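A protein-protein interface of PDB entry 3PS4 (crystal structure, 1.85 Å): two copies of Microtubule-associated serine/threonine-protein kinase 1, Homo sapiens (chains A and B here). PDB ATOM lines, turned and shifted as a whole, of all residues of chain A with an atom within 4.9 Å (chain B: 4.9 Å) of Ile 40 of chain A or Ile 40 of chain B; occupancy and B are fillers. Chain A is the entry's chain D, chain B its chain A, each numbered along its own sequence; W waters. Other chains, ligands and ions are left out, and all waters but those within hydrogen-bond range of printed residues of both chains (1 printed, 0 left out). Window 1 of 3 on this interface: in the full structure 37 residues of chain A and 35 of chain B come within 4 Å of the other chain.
The backbone NH (N) of Trp 42 of chain B is in hydrogen-bond range of the backbone carbonyl oxygen (O) of Thr 21 of chain B (2.8 Å). The backbone NH (N) of Ile 25 of chain B is in hydrogen-bond range of the backbone carbonyl oxygen (O) of His 38 of chain B, 2.8 Å away. N of Trp 42 of chain A lies within hydrogen-bond range of O of Thr 21 of chain A (2.8 Å). N of Arg 23 of chain A sits at hydrogen-bond distance from O of Ile 40 of chain A, 2.8 Å away. The backbone NH of Ile 25 of chain A is in hydrogen-bond range of the backbone carbonyl oxygen of His 38 of chain A (2.8 Å). The backbone carbonyl oxygen (O) of Val 41 of chain A lies within hydrogen-bond range of the backbone NH (N) of Gly 58 of chain A (2.7 Å).
Printed residues of chain B within 4 Å of Ile 40 of chain A: Ile 40 and Trp 42. Of the printed residues of chain A, Ile 40 of chain B touches Ile 40 (3.99 Å). Printed residues of chain B within 4 Å of Leu 60 of chain A: Ile 25. Printed residues of chain A within 4 Å of Ile 25 of chain B: Ile 25 and Leu 60. Of the printed residues of chain B, Val 41 of chain A touches Trp 42. Of the printed residues of chain B, Trp 42 of chain A touches Trp 42 (3.6 Å) and Gly 58 (3.7 Å). Printed residues of chain B within 4 Å of Ile 25 of chain A: Ile 25 (3.5 Å). Ile 61 of chain A touches none of the printed residues of chain B. The nearest printed residue of chain B that does not touch Ile 40 of chain A is Ile 25 of chain B (4.1 Å). The nearest printed residue of chain A that does not touch Ile 40 of chain B is Ile 25 of chain A (4.02 Å). The nearest printed residue of chain A that does not touch Gly 58 of chain B is Ile 25 of chain A (4.2 Å).
Of the 13 printed residues of chain B, 4 touch a printed residue of chain A. Of the 13 printed residues of chain A, 7 touch a printed residue of chain B. Printed residues of chain A that touch a printed residue of chain B: Arg 23, Ile 25, Ile 40, Val 41, Trp 42, Gly 58 and Leu 60. Among the printed residues, no Asp or Glu carboxylate lies within 4 Å of a Lys or Arg side-chain nitrogen of the other chain.
Arg 23 of chain A touches Gly 58 of chain B, but with the chains exchanged Gly 58 of chain A does not touch Arg 23 of chain B (4.1 Å). Ile 40 of chain B touches its own counterpart, Ile 40 of chain A. Val 41 of chain A touches Trp 42 of chain B, but with the chains exchanged Trp 42 of chain A does not touch Val 41 of chain B (4.4 Å). Leu 60 of chain A touches Ile 25 of chain B, but with the chains exchanged Ile 25 of chain A does not touch Leu 60 of chain B (4.8 Å). 12 positions are printed for both chains.
Arg 23 of chain A touches Gly 58 of chain B (NH1 to CA, 3.9 Å). Ile 25 of chain A touches Ile 25 of chain B (CD1 to CD1, 3.5 Å). Ile 40 of chain B touches Ile 40 of chain A (CD1 to CD1, 3.99 Å). Ile 40 of chain A touches Trp 42 of chain B (CD1 to CZ3, 3.99 Å). Val 41 of chain A touches Trp 42 of chain B. CZ3 of Trp 42 of chain B touches CZ3 of Trp 42 of chain A, 3.6 Å away. Trp 42 of chain A touches Gly 58 of chain B (CH2 to N, 3.7 Å). N of Gly 58 of chain A touches CH2 of Trp 42 of chain B, 3.3 Å away. Ile 25 of chain B touches Leu 60 of chain A.
Water W1 lies within hydrogen-bond range of the guanidinium group of Arg 23 of chain B and the side-chain carboxylate of Asp 59 of chain A.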
ATOM      1  N   THR A  21      20.744  17.674  23.416  1.00  0.00           N
ATOM      2  CA  THR A  21      22.056  17.641  22.782  1.00  0.00           C
ATOM      3  C   THR A  21      22.627  19.039  22.776  1.00  0.00           C
ATOM      4  O   THR A  21      21.966  19.983  22.334  1.00  0.00           O
ATOM      5  CB  THR A  21      21.978  17.068  21.368  1.00  0.00           C
ATOM      6  OG1 THR A  21      21.391  15.771  21.449  1.00  0.00           O
ATOM      7  CG2 THR A  21      23.362  16.978  20.693  1.00  0.00           C
ATOM      8  N   LEU A  22      23.863  19.155  23.236  1.00  0.00           N
ATOM      9  CA  LEU A  22      24.570  20.407  23.328  1.00  0.00           C
ATOM     10  C   LEU A  22      25.636  20.440  22.286  1.00  0.00           C
ATOM     11  O   LEU A  22      26.409  19.495  22.167  1.00  0.00           O
ATOM     12  CB  LEU A  22      25.162  20.540  24.744  1.00  0.00           C
ATOM     13  CG  LEU A  22      25.549  21.927  25.223  1.00  0.00           C
ATOM     14  CD1 LEU A  22      24.352  22.893  25.278  1.00  0.00           C
ATOM     15  CD2 LEU A  22      26.173  21.837  26.568  1.00  0.00           C
ATOM     16  N   ARG A  23      25.602  21.491  21.469  1.00  0.00           N
ATOM     17  CA  ARG A  23      26.551  21.724  20.392  1.00  0.00           C
ATOM     18  C   ARG A  23      27.364  22.977  20.696  1.00  0.00           C
ATOM     19  O   ARG A  23      26.825  23.950  21.207  1.00  0.00           O
ATOM     20  CB  ARG A  23      25.793  21.851  19.050  1.00  0.00           C
ATOM     21  CG  ARG A  23      26.534  22.496  17.867  1.00  0.00           C
ATOM     22  CD  ARG A  23      27.534  21.580  17.202  1.00  0.00           C
ATOM     23  NE  ARG A  23      26.886  20.615  16.317  1.00  0.00           N
ATOM     24  CZ  ARG A  23      26.753  20.767  15.004  1.00  0.00           C
ATOM     25  NH1 ARG A  23      27.242  21.846  14.400  1.00  0.00           N
ATOM     26  NH2 ARG A  23      26.148  19.835  14.281  1.00  0.00           N
ATOM     27  N   ILE A  25      29.383  26.231  19.279  1.00  0.00           N
ATOM     28  CA  ILE A  25      29.499  27.059  18.085  1.00  0.00           C
ATOM     29  C   ILE A  25      30.589  28.110  18.320  1.00  0.00           C
ATOM     30  O   ILE A  25      30.741  28.616  19.434  1.00  0.00           O
ATOM     31  CB  ILE A  25      28.159  27.683  17.611  1.00  0.00           C
ATOM     32  CG1 ILE A  25      27.497  28.523  18.705  1.00  0.00           C
ATOM     33  CG2 ILE A  25      27.207  26.597  17.052  1.00  0.00           C
ATOM     34  CD1 ILE A  25      26.625  29.616  18.233  1.00  0.00           C
ATOM     35  N   HIS A  38      30.350  29.222  22.212  1.00  0.00           N
ATOM     36  CA  HIS A  38      28.998  29.353  22.767  1.00  0.00           C
ATOM     37  C   HIS A  38      28.285  28.017  22.627  1.00  0.00           C
ATOM     38  O   HIS A  38      28.663  27.197  21.791  1.00  0.00           O
ATOM     39  CB  HIS A  38      28.239  30.507  22.144  1.00  0.00           C
ATOM     40  CG  HIS A  38      28.852  31.813  22.526  1.00  0.00           C
ATOM     41  ND1 HIS A  38      29.894  32.350  21.801  1.00  0.00           N
ATOM     42  CD2 HIS A  38      28.624  32.594  23.606  1.00  0.00           C
ATOM     43  CE1 HIS A  38      30.226  33.469  22.422  1.00  0.00           C
ATOM     44  NE2 HIS A  38      29.489  33.657  23.514  1.00  0.00           N
ATOM     45  N   HIS A  39      27.309  27.777  23.487  1.00  0.00           N
ATOM     46  CA  HIS A  39      26.691  26.482  23.689  1.00  0.00           C
ATOM     47  C   HIS A  39      25.245  26.525  23.298  1.00  0.00           C
ATOM     48  O   HIS A  39      24.432  27.202  23.925  1.00  0.00           O
ATOM     49  CB  HIS A  39      26.904  26.065  25.162  1.00  0.00           C
ATOM     50  CG  HIS A  39      28.362  26.160  25.534  1.00  0.00           C
ATOM     51  ND1 HIS A  39      29.287  25.195  25.142  1.00  0.00           N
ATOM     52  CD2 HIS A  39      29.033  27.182  26.112  1.00  0.00           C
ATOM     53  CE1 HIS A  39      30.473  25.640  25.539  1.00  0.00           C
ATOM     54  NE2 HIS A  39      30.371  26.830  26.132  1.00  0.00           N
ATOM     55  N   ILE A  40      24.937  25.853  22.202  1.00  0.00           N
ATOM     56  CA  ILE A  40      23.582  25.866  21.658  1.00  0.00           C
ATOM     57  C   ILE A  40      22.909  24.494  21.856  1.00  0.00           C
ATOM     58  O   ILE A  40      23.558  23.449  21.731  1.00  0.00           O
ATOM     59  CB  ILE A  40      23.622  26.300  20.166  1.00  0.00           C
ATOM     60  CG1 ILE A  40      22.217  26.595  19.606  1.00  0.00           C
ATOM     61  CG2 ILE A  40      24.411  25.296  19.272  1.00  0.00           C
ATOM     62  CD1 ILE A  40      22.209  27.439  18.245  1.00  0.00           C
ATOM     63  N   VAL A  41      21.612  24.527  22.165  1.00  0.00           N
ATOM     64  CA  VAL A  41      20.766  23.329  22.267  1.00  0.00           C
ATOM     65  C   VAL A  41      20.486  22.906  20.828  1.00  0.00           C
ATOM     66  O   VAL A  41      19.748  23.561  20.077  1.00  0.00           O
ATOM     67  CB  VAL A  41      19.475  23.549  23.086  1.00  0.00           C
ATOM     68  CG1 VAL A  41      18.652  22.256  23.151  1.00  0.00           C
ATOM     69  CG2 VAL A  41      19.777  24.070  24.492  1.00  0.00           C
ATOM     70  N   TRP A  42      21.140  21.861  20.425  1.00  0.00           N
ATOM     71  CA  TRP A  42      21.023  21.387  19.056  1.00  0.00           C
ATOM     72  C   TRP A  42      19.772  20.552  18.834  1.00  0.00           C
ATOM     73  O   TRP A  42      19.242  20.527  17.719  1.00  0.00           O
ATOM     74  CB  TRP A  42      22.253  20.556  18.701  1.00  0.00           C
ATOM     75  CG  TRP A  42      22.410  20.364  17.218  1.00  0.00           C
ATOM     76  CD1 TRP A  42      22.357  19.194  16.523  1.00  0.00           C
ATOM     77  CD2 TRP A  42      22.658  21.398  16.254  1.00  0.00           C
ATOM     78  NE1 TRP A  42      22.590  19.432  15.179  1.00  0.00           N
ATOM     79  CE2 TRP A  42      22.774  20.778  14.991  1.00  0.00           C
ATOM     80  CE3 TRP A  42      22.863  22.789  16.346  1.00  0.00           C
ATOM     81  CZ2 TRP A  42      23.024  21.506  13.825  1.00  0.00           C
ATOM     82  CZ3 TRP A  42      23.135  23.509  15.192  1.00  0.00           C
ATOM     83  CH2 TRP A  42      23.222  22.868  13.951  1.00  0.00           C
ATOM     84  N   GLY A  58      17.713  25.301  19.532  1.00  0.00           N
ATOM     85  CA  GLY A  58      18.025  26.647  19.063  1.00  0.00           C
ATOM     86  C   GLY A  58      18.311  27.593  20.203  1.00  0.00           C
ATOM     87  O   GLY A  58      18.919  28.635  19.983  1.00  0.00           O
ATOM     88  N   ASP A  59      17.881  27.233  21.434  1.00  0.00           N
ATOM     89  CA  ASP A  59      18.196  28.022  22.631  1.00  0.00           C
ATOM     90  C   ASP A  59      19.699  27.982  22.878  1.00  0.00           C
ATOM     91  O   ASP A  59      20.326  26.921  22.676  1.00  0.00           O
ATOM     92  CB  ASP A  59      17.497  27.418  23.878  1.00  0.00           C
ATOM     93  CG  ASP A  59      15.999  27.574  24.000  1.00  0.00           C
ATOM     94  OD1 ASP A  59      15.424  28.392  23.242  1.00  0.00           O
ATOM     95  OD2 ASP A  59      15.394  26.870  24.854  1.00  0.00           O
ATOM     96  N   LEU A  60      20.303  29.108  23.256  1.00  0.00           N
ATOM     97  CA  LEU A  60      21.706  29.065  23.658  1.00  0.00           C
ATOM     98  C   LEU A  60      21.720  29.051  25.175  1.00  0.00           C
ATOM     99  O   LEU A  60      20.891  29.723  25.785  1.00  0.00           O
ATOM    100  CB  LEU A  60      22.544  30.226  23.106  1.00  0.00           C
ATOM    101  CG  LEU A  60      23.016  30.064  21.677  1.00  0.00           C
ATOM    102  CD1 LEU A  60      21.909  30.451  20.692  1.00  0.00           C
ATOM    103  CD2 LEU A  60      24.271  30.878  21.439  1.00  0.00           C
ATOM    104  N   ILE A  61      22.609  28.266  25.781  1.00  0.00           N
ATOM    105  CA  ILE A  61      22.718  28.201  27.241  1.00  0.00           C
ATOM    106  C   ILE A  61      23.788  29.204  27.662  1.00  0.00           C
ATOM    107  O   ILE A  61      24.933  29.099  27.226  1.00  0.00           O
ATOM    108  CB  ILE A  61      23.023  26.755  27.709  1.00  0.00           C
ATOM    109  CG1 ILE A  61      21.773  25.836  27.444  1.00  0.00           C
ATOM    110  CG2 ILE A  61      23.450  26.732  29.205  1.00  0.00           C
ATOM    111  CD1 ILE A  61      21.998  24.386  27.680  1.00  0.00           C
ATOM    112  N   THR B  21      18.516  26.093   5.824  1.00  0.00           N
ATOM    113  CA  THR B  21      17.632  26.848   6.710  1.00  0.00           C
ATOM    114  C   THR B  21      18.447  27.804   7.509  1.00  0.00           C
ATOM    115  O   THR B  21      19.453  27.421   8.097  1.00  0.00           O
ATOM    116  CB  THR B  21      16.854  25.887   7.607  1.00  0.00           C
ATOM    117  OG1 THR B  21      16.139  25.002   6.762  1.00  0.00           O
ATOM    118  CG2 THR B  21      15.868  26.624   8.563  1.00  0.00           C
ATOM    119  N   LEU B  22      17.994  29.050   7.564  1.00  0.00           N
ATOM    120  CA  LEU B  22      18.650  30.063   8.375  1.00  0.00           C
ATOM    121  C   LEU B  22      17.857  30.387   9.659  1.00  0.00           C
ATOM    122  O   LEU B  22      16.636  30.486   9.617  1.00  0.00           O
ATOM    123  CB  LEU B  22      18.776  31.350   7.566  1.00  0.00           C
ATOM    124  CG  LEU B  22      20.073  31.705   6.929  1.00  0.00           C
ATOM    125  CD1 LEU B  22      19.865  32.972   6.158  1.00  0.00           C
ATOM    126  CD2 LEU B  22      21.187  31.898   7.966  1.00  0.00           C
ATOM    127  N   ARG B  23      18.553  30.642  10.759  1.00  0.00           N
ATOM    128  CA  ARG B  23      17.974  31.144  12.006  1.00  0.00           C
ATOM    129  C   ARG B  23      18.854  32.276  12.495  1.00  0.00           C
ATOM    130  O   ARG B  23      20.041  32.337  12.142  1.00  0.00           O
ATOM    131  CB  ARG B  23      17.883  30.046  13.091  1.00  0.00           C
ATOM    132  CG  ARG B  23      16.711  29.115  12.980  1.00  0.00           C
ATOM    133  CD  ARG B  23      16.591  28.217  14.211  1.00  0.00           C
ATOM    134  NE  ARG B  23      15.985  28.913  15.345  1.00  0.00           N
ATOM    135  CZ  ARG B  23      15.257  28.329  16.291  1.00  0.00           C
ATOM    136  NH1 ARG B  23      15.028  27.023  16.252  1.00  0.00           N
ATOM    137  NH2 ARG B  23      14.743  29.048  17.277  1.00  0.00           N
ATOM    138  N   ALA B  24      18.290  33.155  13.311  1.00  0.00           N
ATOM    139  CA  ALA B  24      19.030  34.239  13.969  1.00  0.00           C
ATOM    140  C   ALA B  24      19.198  33.870  15.418  1.00  0.00           C
ATOM    141  O   ALA B  24      18.244  33.384  16.024  1.00  0.00           O
ATOM    142  CB  ALA B  24      18.302  35.571  13.842  1.00  0.00           C
ATOM    143  N   ILE B  25      20.402  34.024  15.956  1.00  0.00           N
ATOM    144  CA  ILE B  25      20.659  33.651  17.344  1.00  0.00           C
ATOM    145  C   ILE B  25      21.267  34.826  18.095  1.00  0.00           C
ATOM    146  O   ILE B  25      22.037  35.599  17.523  1.00  0.00           O
ATOM    147  CB  ILE B  25      21.549  32.378  17.471  1.00  0.00           C
ATOM    148  CG1 ILE B  25      22.877  32.524  16.700  1.00  0.00           C
ATOM    149  CG2 ILE B  25      20.787  31.092  17.112  1.00  0.00           C
ATOM    150  CD1 ILE B  25      24.008  31.719  17.252  1.00  0.00           C
ATOM    151  N   HIS B  38      23.604  36.855  15.447  1.00  0.00           N
ATOM    152  CA  HIS B  38      24.360  36.087  14.477  1.00  0.00           C
ATOM    153  C   HIS B  38      23.410  35.241  13.655  1.00  0.00           C
ATOM    154  O   HIS B  38      22.308  34.944  14.103  1.00  0.00           O
ATOM    155  CB  HIS B  38      25.428  35.246  15.194  1.00  0.00           C
ATOM    156  CG  HIS B  38      26.505  36.100  15.784  1.00  0.00           C
ATOM    157  ND1 HIS B  38      26.384  36.625  17.053  1.00  0.00           N
ATOM    158  CD2 HIS B  38      27.628  36.592  15.217  1.00  0.00           C
ATOM    159  CE1 HIS B  38      27.459  37.374  17.235  1.00  0.00           C
ATOM    160  NE2 HIS B  38      28.235  37.386  16.157  1.00  0.00           N
ATOM    161  N   HIS B  39      23.819  34.899  12.433  1.00  0.00           N
ATOM    162  CA  HIS B  39      23.008  34.151  11.473  1.00  0.00           C
ATOM    163  C   HIS B  39      23.579  32.761  11.282  1.00  0.00           C
ATOM    164  O   HIS B  39      24.676  32.591  10.753  1.00  0.00           O
ATOM    165  CB  HIS B  39      22.925  34.948  10.157  1.00  0.00           C
ATOM    166  CG  HIS B  39      22.389  36.320  10.379  1.00  0.00           C
ATOM    167  ND1 HIS B  39      21.037  36.526  10.513  1.00  0.00           N
ATOM    168  CD2 HIS B  39      23.030  37.503  10.521  1.00  0.00           C
ATOM    169  CE1 HIS B  39      20.891  37.819  10.712  1.00  0.00           C
ATOM    170  NE2 HIS B  39      22.058  38.446  10.726  1.00  0.00           N
ATOM    171  N   ILE B  40      22.865  31.772  11.782  1.00  0.00           N
ATOM    172  CA  ILE B  40      23.336  30.396  11.757  1.00  0.00           C
ATOM    173  C   ILE B  40      22.609  29.568  10.712  1.00  0.00           C
ATOM    174  O   ILE B  40      21.381  29.696  10.532  1.00  0.00           O
ATOM    175  CB  ILE B  40      23.178  29.768  13.169  1.00  0.00           C
ATOM    176  CG1 ILE B  40      23.871  28.360  13.247  1.00  0.00           C
ATOM    177  CG2 ILE B  40      21.666  29.719  13.641  1.00  0.00           C
ATOM    178  CD1 ILE B  40      24.133  27.825  14.773  1.00  0.00           C
ATOM    179  N   VAL B  41      23.375  28.685  10.073  1.00  0.00           N
ATOM    180  CA  VAL B  41      22.870  27.664   9.186  1.00  0.00           C
ATOM    181  C   VAL B  41      22.352  26.566  10.099  1.00  0.00           C
ATOM    182  O   VAL B  41      23.146  25.791  10.658  1.00  0.00           O
ATOM    183  CB  VAL B  41      23.957  27.153   8.228  1.00  0.00           C
ATOM    184  CG1 VAL B  41      23.373  26.108   7.285  1.00  0.00           C
ATOM    185  CG2 VAL B  41      24.622  28.312   7.463  1.00  0.00           C
ATOM    186  N   TRP B  42      21.041  26.513  10.264  1.00  0.00           N
ATOM    187  CA  TRP B  42      20.383  25.606  11.185  1.00  0.00           C
ATOM    188  C   TRP B  42      20.230  24.202  10.628  1.00  0.00           C
ATOM    189  O   TRP B  42      20.238  23.240  11.397  1.00  0.00           O
ATOM    190  CB  TRP B  42      19.029  26.213  11.531  1.00  0.00           C
ATOM    191  CG  TRP B  42      18.251  25.535  12.605  1.00  0.00           C
ATOM    192  CD1 TRP B  42      16.964  25.111  12.513  1.00  0.00           C
ATOM    193  CD2 TRP B  42      18.673  25.264  13.947  1.00  0.00           C
ATOM    194  NE1 TRP B  42      16.545  24.605  13.714  1.00  0.00           N
ATOM    195  CE2 TRP B  42      17.588  24.646  14.605  1.00  0.00           C
ATOM    196  CE3 TRP B  42      19.861  25.499  14.664  1.00  0.00           C
ATOM    197  CZ2 TRP B  42      17.667  24.205  15.934  1.00  0.00           C
ATOM    198  CZ3 TRP B  42      19.941  25.055  15.980  1.00  0.00           C
ATOM    199  CH2 TRP B  42      18.866  24.378  16.582  1.00  0.00           C
ATOM    200  N   GLY B  58      25.406  24.598  11.519  1.00  0.00           N
ATOM    201  CA  GLY B  58      26.241  25.119  12.594  1.00  0.00           C
ATOM    202  C   GLY B  58      27.153  26.232  12.100  1.00  0.00           C
ATOM    203  O   GLY B  58      27.673  27.005  12.914  1.00  0.00           O
ATOM    204  N   ASP B  59      27.368  26.319  10.756  1.00  0.00           N
ATOM    205  CA  ASP B  59      28.133  27.419  10.158  1.00  0.00           C
ATOM    206  C   ASP B  59      27.456  28.727  10.492  1.00  0.00           C
ATOM    207  O   ASP B  59      26.231  28.772  10.573  1.00  0.00           O
ATOM    208  CB  ASP B  59      28.216  27.295   8.615  1.00  0.00           C
ATOM    209  CG  ASP B  59      29.166  26.235   8.068  1.00  0.00           C
ATOM    210  OD1 ASP B  59      30.017  25.750   8.831  1.00  0.00           O
ATOM    211  OD2 ASP B  59      29.054  25.903   6.864  1.00  0.00           O
ATOM    212  N   LEU B  60      28.241  29.780  10.685  1.00  0.00           N
ATOM    213  CA  LEU B  60      27.679  31.125  10.866  1.00  0.00           C
ATOM    214  C   LEU B  60      27.933  31.891   9.586  1.00  0.00           C
ATOM    215  O   LEU B  60      29.040  31.801   9.058  1.00  0.00           O
ATOM    216  CB  LEU B  60      28.313  31.860  12.075  1.00  0.00           C
ATOM    217  CG  LEU B  60      27.965  31.324  13.467  1.00  0.00           C
ATOM    218  CD1 LEU B  60      28.557  32.238  14.523  1.00  0.00           C
ATOM    219  CD2 LEU B  60      26.471  31.291  13.694  1.00  0.00           C
HETATM  220  O   HOH W   1      14.609  28.229  19.897  1.00  0.00           O
